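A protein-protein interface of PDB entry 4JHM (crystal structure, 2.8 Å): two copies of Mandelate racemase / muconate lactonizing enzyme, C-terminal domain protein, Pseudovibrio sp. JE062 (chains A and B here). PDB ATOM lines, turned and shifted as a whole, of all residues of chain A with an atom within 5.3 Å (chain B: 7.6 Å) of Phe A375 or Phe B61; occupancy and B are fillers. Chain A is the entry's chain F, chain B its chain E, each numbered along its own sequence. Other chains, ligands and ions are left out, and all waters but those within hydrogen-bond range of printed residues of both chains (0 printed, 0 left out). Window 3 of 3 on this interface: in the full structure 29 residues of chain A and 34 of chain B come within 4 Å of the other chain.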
ATOM      1  N   SER A   9     -23.123  28.124  18.101  1.00  0.00           N
ATOM      2  CA  SER A   9     -22.199  29.124  17.563  1.00  0.00           C
ATOM      3  C   SER A   9     -20.826  29.022  18.208  1.00  0.00           C
ATOM      4  O   SER A   9     -19.810  29.297  17.566  1.00  0.00           O
ATOM      5  CB  SER A   9     -22.740  30.533  17.807  1.00  0.00           C
ATOM      6  OG  SER A   9     -24.065  30.667  17.331  1.00  0.00           O
ATOM      7  N   ARG A  10     -20.808  28.633  19.481  1.00  0.00           N
ATOM      8  CA  ARG A  10     -19.594  28.679  20.289  1.00  0.00           C
ATOM      9  C   ARG A  10     -19.734  27.808  21.537  1.00  0.00           C
ATOM     10  O   ARG A  10     -20.828  27.667  22.093  1.00  0.00           O
ATOM     11  CB  ARG A  10     -19.311  30.134  20.679  1.00  0.00           C
ATOM     12  CG  ARG A  10     -18.326  30.351  21.818  1.00  0.00           C
ATOM     13  CD  ARG A  10     -18.482  31.762  22.368  1.00  0.00           C
ATOM     14  NE  ARG A  10     -17.395  32.165  23.260  1.00  0.00           N
ATOM     15  CZ  ARG A  10     -16.352  32.906  22.891  1.00  0.00           C
ATOM     16  NH1 ARG A  10     -16.235  33.328  21.638  1.00  0.00           N
ATOM     17  NH2 ARG A  10     -15.420  33.224  23.777  1.00  0.00           N
ATOM     18  N   VAL A  11     -18.627  27.209  21.965  1.00  0.00           N
ATOM     19  CA  VAL A  11     -18.601  26.491  23.232  1.00  0.00           C
ATOM     20  C   VAL A  11     -17.333  26.831  24.007  1.00  0.00           C
ATOM     21  O   VAL A  11     -16.266  27.033  23.425  1.00  0.00           O
ATOM     22  CB  VAL A  11     -18.689  24.956  23.054  1.00  0.00           C
ATOM     23  CG1 VAL A  11     -19.770  24.591  22.045  1.00  0.00           C
ATOM     24  CG2 VAL A  11     -17.345  24.378  22.638  1.00  0.00           C
ATOM     25  N   GLU A  12     -17.467  26.904  25.324  1.00  0.00           N
ATOM     26  CA  GLU A  12     -16.332  27.147  26.193  1.00  0.00           C
ATOM     27  C   GLU A  12     -16.225  26.017  27.197  1.00  0.00           C
ATOM     28  O   GLU A  12     -17.236  25.527  27.703  1.00  0.00           O
ATOM     29  CB  GLU A  12     -16.491  28.471  26.938  1.00  0.00           C
ATOM     30  CG  GLU A  12     -16.519  29.697  26.044  1.00  0.00           C
ATOM     31  CD  GLU A  12     -16.930  30.939  26.798  1.00  0.00           C
ATOM     32  OE1 GLU A  12     -17.309  31.933  26.143  1.00  0.00           O
ATOM     33  OE2 GLU A  12     -16.880  30.917  28.046  1.00  0.00           O
ATOM     34  N   LEU A  13     -14.991  25.609  27.476  1.00  0.00           N
ATOM     35  CA  LEU A  13     -14.725  24.590  28.478  1.00  0.00           C
ATOM     36  C   LEU A  13     -13.952  25.196  29.640  1.00  0.00           C
ATOM     37  O   LEU A  13     -13.146  26.110  29.462  1.00  0.00           O
ATOM     38  CB  LEU A  13     -13.947  23.428  27.862  1.00  0.00           C
ATOM     39  CG  LEU A  13     -14.672  22.718  26.718  1.00  0.00           C
ATOM     40  CD1 LEU A  13     -13.859  21.537  26.214  1.00  0.00           C
ATOM     41  CD2 LEU A  13     -16.055  22.270  27.166  1.00  0.00           C
ATOM     42  N   ARG A  71     -12.423  18.124  25.073  1.00  0.00           N
ATOM     43  CA  ARG A  71     -11.719  18.860  24.032  1.00  0.00           C
ATOM     44  C   ARG A  71     -11.786  18.139  22.692  1.00  0.00           C
ATOM     45  O   ARG A  71     -11.756  18.778  21.643  1.00  0.00           O
ATOM     46  CB  ARG A  71     -10.259  19.063  24.423  1.00  0.00           C
ATOM     47  CG  ARG A  71      -9.427  19.778  23.372  1.00  0.00           C
ATOM     48  CD  ARG A  71      -8.054  20.130  23.919  1.00  0.00           C
ATOM     49  NE  ARG A  71      -7.334  21.062  23.056  1.00  0.00           N
ATOM     50  CZ  ARG A  71      -6.524  20.694  22.070  1.00  0.00           C
ATOM     51  NH1 ARG A  71      -6.327  19.406  21.806  1.00  0.00           N
ATOM     52  NH2 ARG A  71      -5.915  21.621  21.341  1.00  0.00           N
ATOM     53  N   THR A  72     -11.866  16.810  22.737  1.00  0.00           N
ATOM     54  CA  THR A  72     -11.906  15.995  21.526  1.00  0.00           C
ATOM     55  C   THR A  72     -13.324  15.793  21.032  1.00  0.00           C
ATOM     56  O   THR A  72     -13.538  15.401  19.892  1.00  0.00           O
ATOM     57  CB  THR A  72     -11.303  14.602  21.766  1.00  0.00           C
ATOM     58  OG1 THR A  72     -11.911  14.008  22.920  1.00  0.00           O
ATOM     59  CG2 THR A  72      -9.803  14.700  21.976  1.00  0.00           C
ATOM     60  N   VAL A  74     -16.152  18.181  21.562  1.00  0.00           N
ATOM     61  CA  VAL A  74     -16.994  19.359  21.313  1.00  0.00           C
ATOM     62  C   VAL A  74     -16.783  20.086  19.983  1.00  0.00           C
ATOM     63  O   VAL A  74     -17.691  20.772  19.514  1.00  0.00           O
ATOM     64  CB  VAL A  74     -16.858  20.401  22.446  1.00  0.00           C
ATOM     65  CG1 VAL A  74     -17.243  19.786  23.785  1.00  0.00           C
ATOM     66  CG2 VAL A  74     -15.448  20.979  22.489  1.00  0.00           C
ATOM     67  N   PRO A  75     -15.592  19.965  19.374  1.00  0.00           N
ATOM     68  CA  PRO A  75     -15.405  20.685  18.116  1.00  0.00           C
ATOM     69  C   PRO A  75     -16.504  20.414  17.085  1.00  0.00           C
ATOM     70  O   PRO A  75     -16.892  21.320  16.353  1.00  0.00           O
ATOM     71  CB  PRO A  75     -14.050  20.175  17.623  1.00  0.00           C
ATOM     72  CG  PRO A  75     -13.310  19.856  18.873  1.00  0.00           C
ATOM     73  CD  PRO A  75     -14.348  19.307  19.816  1.00  0.00           C
ATOM     74  N   ILE A  78     -20.272  22.562  16.786  1.00  0.00           N
ATOM     75  CA  ILE A  78     -20.551  23.757  15.992  1.00  0.00           C
ATOM     76  C   ILE A  78     -21.461  23.432  14.812  1.00  0.00           C
ATOM     77  O   ILE A  78     -21.105  22.640  13.942  1.00  0.00           O
ATOM     78  CB  ILE A  78     -19.254  24.398  15.457  1.00  0.00           C
ATOM     79  CG1 ILE A  78     -18.285  24.714  16.605  1.00  0.00           C
ATOM     80  CG2 ILE A  78     -19.573  25.663  14.678  1.00  0.00           C
ATOM     81  CD1 ILE A  78     -18.819  25.700  17.624  1.00  0.00           C
ATOM     82  N   TYR A 373     -10.625  26.208  27.402  1.00  0.00           N
ATOM     83  CA  TYR A 373     -10.624  26.069  25.951  1.00  0.00           C
ATOM     84  C   TYR A 373     -11.792  26.849  25.359  1.00  0.00           C
ATOM     85  O   TYR A 373     -12.834  27.007  25.996  1.00  0.00           O
ATOM     86  CB  TYR A 373     -10.716  24.599  25.535  1.00  0.00           C
ATOM     87  CG  TYR A 373      -9.466  23.807  25.829  1.00  0.00           C
ATOM     88  CD1 TYR A 373      -8.347  23.909  25.009  1.00  0.00           C
ATOM     89  CD2 TYR A 373      -9.400  22.955  26.929  1.00  0.00           C
ATOM     90  CE1 TYR A 373      -7.199  23.187  25.275  1.00  0.00           C
ATOM     91  CE2 TYR A 373      -8.257  22.226  27.201  1.00  0.00           C
ATOM     92  CZ  TYR A 373      -7.159  22.346  26.373  1.00  0.00           C
ATOM     93  OH  TYR A 373      -6.021  21.622  26.641  1.00  0.00           O
ATOM     94  N   VAL A 374     -11.604  27.337  24.138  1.00  0.00           N
ATOM     95  CA  VAL A 374     -12.630  28.099  23.444  1.00  0.00           C
ATOM     96  C   VAL A 374     -12.761  27.582  22.012  1.00  0.00           C
ATOM     97  O   VAL A 374     -11.762  27.283  21.359  1.00  0.00           O
ATOM     98  CB  VAL A 374     -12.294  29.607  23.444  1.00  0.00           C
ATOM     99  CG1 VAL A 374     -11.063  29.886  22.594  1.00  0.00           C
ATOM    100  CG2 VAL A 374     -13.485  30.421  22.962  1.00  0.00           C
ATOM    101  N   PHE A 375     -13.996  27.462  21.536  1.00  0.00           N
ATOM    102  CA  PHE A 375     -14.256  26.936  20.197  1.00  0.00           C
ATOM    103  C   PHE A 375     -15.340  27.748  19.502  1.00  0.00           C
ATOM    104  O   PHE A 375     -16.355  28.091  20.109  1.00  0.00           O
ATOM    105  CB  PHE A 375     -14.674  25.465  20.266  1.00  0.00           C
ATOM    106  CG  PHE A 375     -13.584  24.545  20.742  1.00  0.00           C
ATOM    107  CD1 PHE A 375     -12.530  24.207  19.906  1.00  0.00           C
ATOM    108  CD2 PHE A 375     -13.610  24.021  22.024  1.00  0.00           C
ATOM    109  CE1 PHE A 375     -11.522  23.366  20.340  1.00  0.00           C
ATOM    110  CE2 PHE A 375     -12.606  23.178  22.464  1.00  0.00           C
ATOM    111  CZ  PHE A 375     -11.561  22.848  21.619  1.00  0.00           C
ATOM    112  N   GLU A 376     -15.125  28.046  18.223  1.00  0.00           N
ATOM    113  CA  GLU A 376     -16.030  28.915  17.483  1.00  0.00           C
ATOM    114  C   GLU A 376     -15.953  28.671  15.978  1.00  0.00           C
ATOM    115  O   GLU A 376     -15.147  27.871  15.505  1.00  0.00           O
ATOM    116  CB  GLU A 376     -15.718  30.382  17.805  1.00  0.00           C
ATOM    117  CG  GLU A 376     -14.245  30.755  17.679  1.00  0.00           C
ATOM    118  CD  GLU A 376     -13.946  32.167  18.154  1.00  0.00           C
ATOM    119  OE1 GLU A 376     -12.804  32.630  17.956  1.00  0.00           O
ATOM    120  OE2 GLU A 376     -14.848  32.817  18.726  1.00  0.00           O
ATOM    121  N   GLU A 377     -16.806  29.366  15.233  1.00  0.00           N
ATOM    122  CA  GLU A 377     -16.836  29.265  13.777  1.00  0.00           C
ATOM    123  C   GLU A 377     -16.020  30.392  13.130  1.00  0.00           C
ATOM    124  O   GLU A 377     -16.185  31.566  13.472  1.00  0.00           O
ATOM    125  CB  GLU A 377     -18.287  29.311  13.284  1.00  0.00           C
ATOM    126  CG  GLU A 377     -18.990  30.637  13.549  1.00  0.00           C
ATOM    127  CD  GLU A 377     -20.497  30.505  13.667  1.00  0.00           C
ATOM    128  OE1 GLU A 377     -20.975  29.431  14.087  1.00  0.00           O
ATOM    129  OE2 GLU A 377     -21.203  31.486  13.351  1.00  0.00           O
ATOM    130  N   PRO B  32     -12.730  10.937  10.905  1.00  0.00           N
ATOM    131  CA  PRO B  32     -11.465  10.192  10.971  1.00  0.00           C
ATOM    132  C   PRO B  32     -10.805  10.234  12.352  1.00  0.00           C
ATOM    133  O   PRO B  32     -10.513  11.315  12.865  1.00  0.00           O
ATOM    134  CB  PRO B  32     -10.576  10.897   9.930  1.00  0.00           C
ATOM    135  CG  PRO B  32     -11.280  12.161   9.558  1.00  0.00           C
ATOM    136  CD  PRO B  32     -12.735  11.917   9.804  1.00  0.00           C
ATOM    137  N   LEU B  33     -10.565   9.063  12.939  1.00  0.00           N
ATOM    138  CA  LEU B  33      -9.980   8.977  14.277  1.00  0.00           C
ATOM    139  C   LEU B  33      -8.464   9.173  14.266  1.00  0.00           C
ATOM    140  O   LEU B  33      -7.747   8.530  13.498  1.00  0.00           O
ATOM    141  CB  LEU B  33     -10.292   7.624  14.919  1.00  0.00           C
ATOM    142  CG  LEU B  33     -11.761   7.257  15.127  1.00  0.00           C
ATOM    143  CD1 LEU B  33     -11.862   5.804  15.562  1.00  0.00           C
ATOM    144  CD2 LEU B  33     -12.438   8.171  16.137  1.00  0.00           C
ATOM    145  N   LEU B  34      -7.990  10.064  15.134  1.00  0.00           N
ATOM    146  CA  LEU B  34      -6.565  10.279  15.331  1.00  0.00           C
ATOM    147  C   LEU B  34      -6.077   9.369  16.453  1.00  0.00           C
ATOM    148  O   LEU B  34      -6.714   9.269  17.504  1.00  0.00           O
ATOM    149  CB  LEU B  34      -6.297  11.742  15.689  1.00  0.00           C
ATOM    150  CG  LEU B  34      -6.333  12.772  14.553  1.00  0.00           C
ATOM    151  CD1 LEU B  34      -7.353  12.403  13.485  1.00  0.00           C
ATOM    152  CD2 LEU B  34      -6.614  14.161  15.108  1.00  0.00           C
ATOM    153  N   TYR B  35      -4.944   8.711  16.234  1.00  0.00           N
ATOM    154  CA  TYR B  35      -4.434   7.736  17.195  1.00  0.00           C
ATOM    155  C   TYR B  35      -3.303   8.287  18.061  1.00  0.00           C
ATOM    156  O   TYR B  35      -2.570   9.187  17.655  1.00  0.00           O
ATOM    157  CB  TYR B  35      -4.000   6.458  16.475  1.00  0.00           C
ATOM    158  CG  TYR B  35      -5.176   5.604  16.051  1.00  0.00           C
ATOM    159  CD1 TYR B  35      -6.062   6.049  15.080  1.00  0.00           C
ATOM    160  CD2 TYR B  35      -5.413   4.360  16.635  1.00  0.00           C
ATOM    161  CE1 TYR B  35      -7.146   5.284  14.695  1.00  0.00           C
ATOM    162  CE2 TYR B  35      -6.494   3.586  16.251  1.00  0.00           C
ATOM    163  CZ  TYR B  35      -7.356   4.055  15.280  1.00  0.00           C
ATOM    164  OH  TYR B  35      -8.435   3.302  14.884  1.00  0.00           O
ATOM    165  N   THR B  36      -3.182   7.736  19.262  1.00  0.00           N
ATOM    166  CA  THR B  36      -2.205   8.194  20.238  1.00  0.00           C
ATOM    167  C   THR B  36      -1.733   7.015  21.073  1.00  0.00           C
ATOM    168  O   THR B  36      -2.539   6.176  21.482  1.00  0.00           O
ATOM    169  CB  THR B  36      -2.821   9.232  21.198  1.00  0.00           C
ATOM    170  OG1 THR B  36      -3.279  10.370  20.457  1.00  0.00           O
ATOM    171  CG2 THR B  36      -1.804   9.678  22.237  1.00  0.00           C
ATOM    172  N   TYR B  57      -8.032   6.470  20.689  1.00  0.00           N
ATOM    173  CA  TYR B  57      -8.547   6.859  19.382  1.00  0.00           C
ATOM    174  C   TYR B  57      -9.528   8.011  19.564  1.00  0.00           C
ATOM    175  O   TYR B  57     -10.533   7.884  20.262  1.00  0.00           O
ATOM    176  CB  TYR B  57      -9.197   5.675  18.652  1.00  0.00           C
ATOM    177  CG  TYR B  57      -9.911   4.676  19.543  1.00  0.00           C
ATOM    178  CD1 TYR B  57      -9.228   3.604  20.106  1.00  0.00           C
ATOM    179  CD2 TYR B  57     -11.273   4.794  19.805  1.00  0.00           C
ATOM    180  CE1 TYR B  57      -9.876   2.685  20.914  1.00  0.00           C
ATOM    181  CE2 TYR B  57     -11.930   3.878  20.612  1.00  0.00           C
ATOM    182  CZ  TYR B  57     -11.226   2.826  21.163  1.00  0.00           C
ATOM    183  OH  TYR B  57     -11.871   1.910  21.964  1.00  0.00           O
ATOM    184  N   THR B  58      -9.211   9.144  18.945  1.00  0.00           N
ATOM    185  CA  THR B  58      -9.995  10.362  19.113  1.00  0.00           C
ATOM    186  C   THR B  58     -10.166  11.098  17.801  1.00  0.00           C
ATOM    187  O   THR B  58      -9.520  10.779  16.805  1.00  0.00           O
ATOM    188  CB  THR B  58      -9.309  11.332  20.086  1.00  0.00           C
ATOM    189  OG1 THR B  58      -7.952  11.543  19.666  1.00  0.00           O
ATOM    190  CG2 THR B  58      -9.334  10.775  21.497  1.00  0.00           C
ATOM    191  N   GLU B  59     -11.035  12.098  17.815  1.00  0.00           N
ATOM    192  CA  GLU B  59     -11.258  12.929  16.646  1.00  0.00           C
ATOM    193  C   GLU B  59     -10.704  14.325  16.894  1.00  0.00           C
ATOM    194  O   GLU B  59     -10.365  14.677  18.026  1.00  0.00           O
ATOM    195  CB  GLU B  59     -12.752  13.004  16.335  1.00  0.00           C
ATOM    196  CG  GLU B  59     -13.415  11.646  16.166  1.00  0.00           C
ATOM    197  CD  GLU B  59     -14.900  11.749  15.874  1.00  0.00           C
ATOM    198  OE1 GLU B  59     -15.424  12.882  15.836  1.00  0.00           O
ATOM    199  OE2 GLU B  59     -15.544  10.693  15.678  1.00  0.00           O
ATOM    200  N   ASN B  60     -10.599  15.106  15.824  1.00  0.00           N
ATOM    201  CA  ASN B  60     -10.220  16.516  15.913  1.00  0.00           C
ATOM    202  C   ASN B  60      -8.771  16.723  16.345  1.00  0.00           C
ATOM    203  O   ASN B  60      -8.003  17.385  15.644  1.00  0.00           O
ATOM    204  CB  ASN B  60     -11.167  17.260  16.862  1.00  0.00           C
ATOM    205  CG  ASN B  60     -12.632  16.996  16.549  1.00  0.00           C
ATOM    206  OD1 ASN B  60     -13.067  17.135  15.407  1.00  0.00           O
ATOM    207  ND2 ASN B  60     -13.397  16.607  17.565  1.00  0.00           N
ATOM    208  N   PHE B  61      -8.405  16.169  17.500  1.00  0.00           N
ATOM    209  CA  PHE B  61      -7.049  16.313  18.031  1.00  0.00           C
ATOM    210  C   PHE B  61      -6.539  14.995  18.593  1.00  0.00           C
ATOM    211  O   PHE B  61      -7.303  14.042  18.754  1.00  0.00           O
ATOM    212  CB  PHE B  61      -7.009  17.370  19.140  1.00  0.00           C
ATOM    213  CG  PHE B  61      -7.826  18.592  18.845  1.00  0.00           C
ATOM    214  CD1 PHE B  61      -7.343  19.578  18.002  1.00  0.00           C
ATOM    215  CD2 PHE B  61      -9.081  18.757  19.414  1.00  0.00           C
ATOM    216  CE1 PHE B  61      -8.096  20.705  17.728  1.00  0.00           C
ATOM    217  CE2 PHE B  61      -9.840  19.880  19.143  1.00  0.00           C
ATOM    218  CZ  PHE B  61      -9.345  20.857  18.300  1.00  0.00           C
ATOM    219  N   PHE B  62      -5.245  14.954  18.900  1.00  0.00           N
ATOM    220  CA  PHE B  62      -4.650  13.806  19.576  1.00  0.00           C
ATOM    221  C   PHE B  62      -5.034  13.840  21.050  1.00  0.00           C
ATOM    222  O   PHE B  62      -5.120  14.910  21.646  1.00  0.00           O
ATOM    223  CB  PHE B  62      -3.130  13.807  19.402  1.00  0.00           C
ATOM    224  CG  PHE B  62      -2.688  13.668  17.972  1.00  0.00           C
ATOM    225  CD1 PHE B  62      -2.841  12.464  17.300  1.00  0.00           C
ATOM    226  CD2 PHE B  62      -2.127  14.741  17.295  1.00  0.00           C
ATOM    227  CE1 PHE B  62      -2.444  12.331  15.982  1.00  0.00           C
ATOM    228  CE2 PHE B  62      -1.725  14.616  15.977  1.00  0.00           C
ATOM    229  CZ  PHE B  62      -1.883  13.410  15.319  1.00  0.00           C
ATOM    230  N   ASP B  63      -5.273  12.668  21.633  1.00  0.00           N
ATOM    231  CA  ASP B  63      -5.847  12.575  22.973  1.00  0.00           C
ATOM    232  C   ASP B  63      -4.821  12.889  24.055  1.00  0.00           C
ATOM    233  O   ASP B  63      -3.701  12.378  24.031  1.00  0.00           O
ATOM    234  CB  ASP B  63      -6.419  11.172  23.204  1.00  0.00           C
ATOM    235  CG  ASP B  63      -7.431  11.124  24.343  1.00  0.00           C
ATOM    236  OD1 ASP B  63      -8.065  12.165  24.633  1.00  0.00           O
ATOM    237  OD2 ASP B  63      -7.605  10.036  24.939  1.00  0.00           O
ATOM    238  N   ARG B  64      -5.207  13.739  25.001  1.00  0.00           N
ATOM    239  CA  ARG B  64      -4.411  13.956  26.203  1.00  0.00           C
ATOM    240  C   ARG B  64      -5.162  13.447  27.437  1.00  0.00           C
ATOM    241  O   ARG B  64      -4.621  13.401  28.538  1.00  0.00           O
ATOM    242  CB  ARG B  64      -4.058  15.438  26.353  1.00  0.00           C
ATOM    243  CG  ARG B  64      -2.768  15.847  25.657  1.00  0.00           C
ATOM    244  CD  ARG B  64      -2.307  17.220  26.115  1.00  0.00           C
ATOM    245  NE  ARG B  64      -3.046  18.292  25.454  1.00  0.00           N
ATOM    246  CZ  ARG B  64      -2.562  19.048  24.472  1.00  0.00           C
ATOM    247  NH1 ARG B  64      -3.318  19.998  23.935  1.00  0.00           N
ATOM    248  NH2 ARG B  64      -1.324  18.866  24.025  1.00  0.00           N
ATOM    249  N   PHE B 370       3.968  14.937  22.149  1.00  0.00           N
ATOM    250  CA  PHE B 370       3.421  16.290  22.198  1.00  0.00           C
ATOM    251  C   PHE B 370       2.956  16.632  23.609  1.00  0.00           C
ATOM    252  O   PHE B 370       2.453  17.724  23.858  1.00  0.00           O
ATOM    253  CB  PHE B 370       2.253  16.433  21.220  1.00  0.00           C
ATOM    254  CG  PHE B 370       1.137  15.460  21.464  1.00  0.00           C
ATOM    255  CD1 PHE B 370       0.173  15.717  22.424  1.00  0.00           C
ATOM    256  CD2 PHE B 370       1.057  14.282  20.736  1.00  0.00           C
ATOM    257  CE1 PHE B 370      -0.854  14.816  22.651  1.00  0.00           C
ATOM    258  CE2 PHE B 370       0.033  13.379  20.959  1.00  0.00           C
ATOM    259  CZ  PHE B 370      -0.924  13.646  21.919  1.00  0.00           C
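The side-chain amide nitrogen of Asn B60 is in hydrogen-bond range of the backbone carbonyl oxygen of Thr A72 (2.6 Å).
N of Phe A375 is in hydrogen-bond range of O of Val A11 (3.0 Å). OG1 of Thr B58 is in hydrogen-bond range of O of Phe B61. N of Thr B58 is in hydrogen-bond range of O of Leu B34 (2.9 Å).
Of the 14 printed residues of chain B, 5 touch a printed residue of chain A. Printed residues of chain B that touch a printed residue of chain A: Thr B58, Glu B59, Asn B60, Phe B61 and Arg B64. Hydrophobic or aromatic side chains of chain B within 4 Å of the printed part of chain A: Phe B61. Of the 15 printed residues of chain A, 4 touch a printed residue of chain B. Hydrophobic or aromatic side chains of chain A within 4 Å of the printed part of chain B: Pro A75 and Phe A375. Among the printed residues, 8 pairs touch across the chains.
Among the printed residues, merely in contact across the chains: Arg A71 with Phe B61, Arg A71 with Arg B64, Thr A72 with Thr B58, Thr A72 with Glu B59, Pro A75 with Asn B60, Pro A75 with Phe B61 and Phe A375 with Phe B61.
Phe A375 touches just one residue of chain B: Phe B61. Printed residues of chain A within 4 Å of Asn B60: Thr A72 (2.6 Å) and Pro A75 (3.5 Å). Of the printed residues of chain B, Pro A75 touches Asn B60 (3.5 Å) and Phe B61 (3.5 Å). Of the printed residues of chain B, Thr A72 touches Thr B58 (3.9 Å), Glu B59 (3.8 Å) and Asn B60 (2.6 Å). Printed residues of chain A within 4 Å of Thr B58: Thr A72. Leu B33 touches none of the printed residues of chain A. Phe B62 touches none of the printed residues of chain A. The nearest residue of chain B that does not touch Phe A375 is Asn B60 (7.0 Å). The nearest residue of chain A that does not touch Phe B61 is Thr A72 (4.1 Å).
No position is printed for both chains. Of the 8 pairs that touch across the chains among the printed residues, none has its exchanged pair printed and touching as well.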
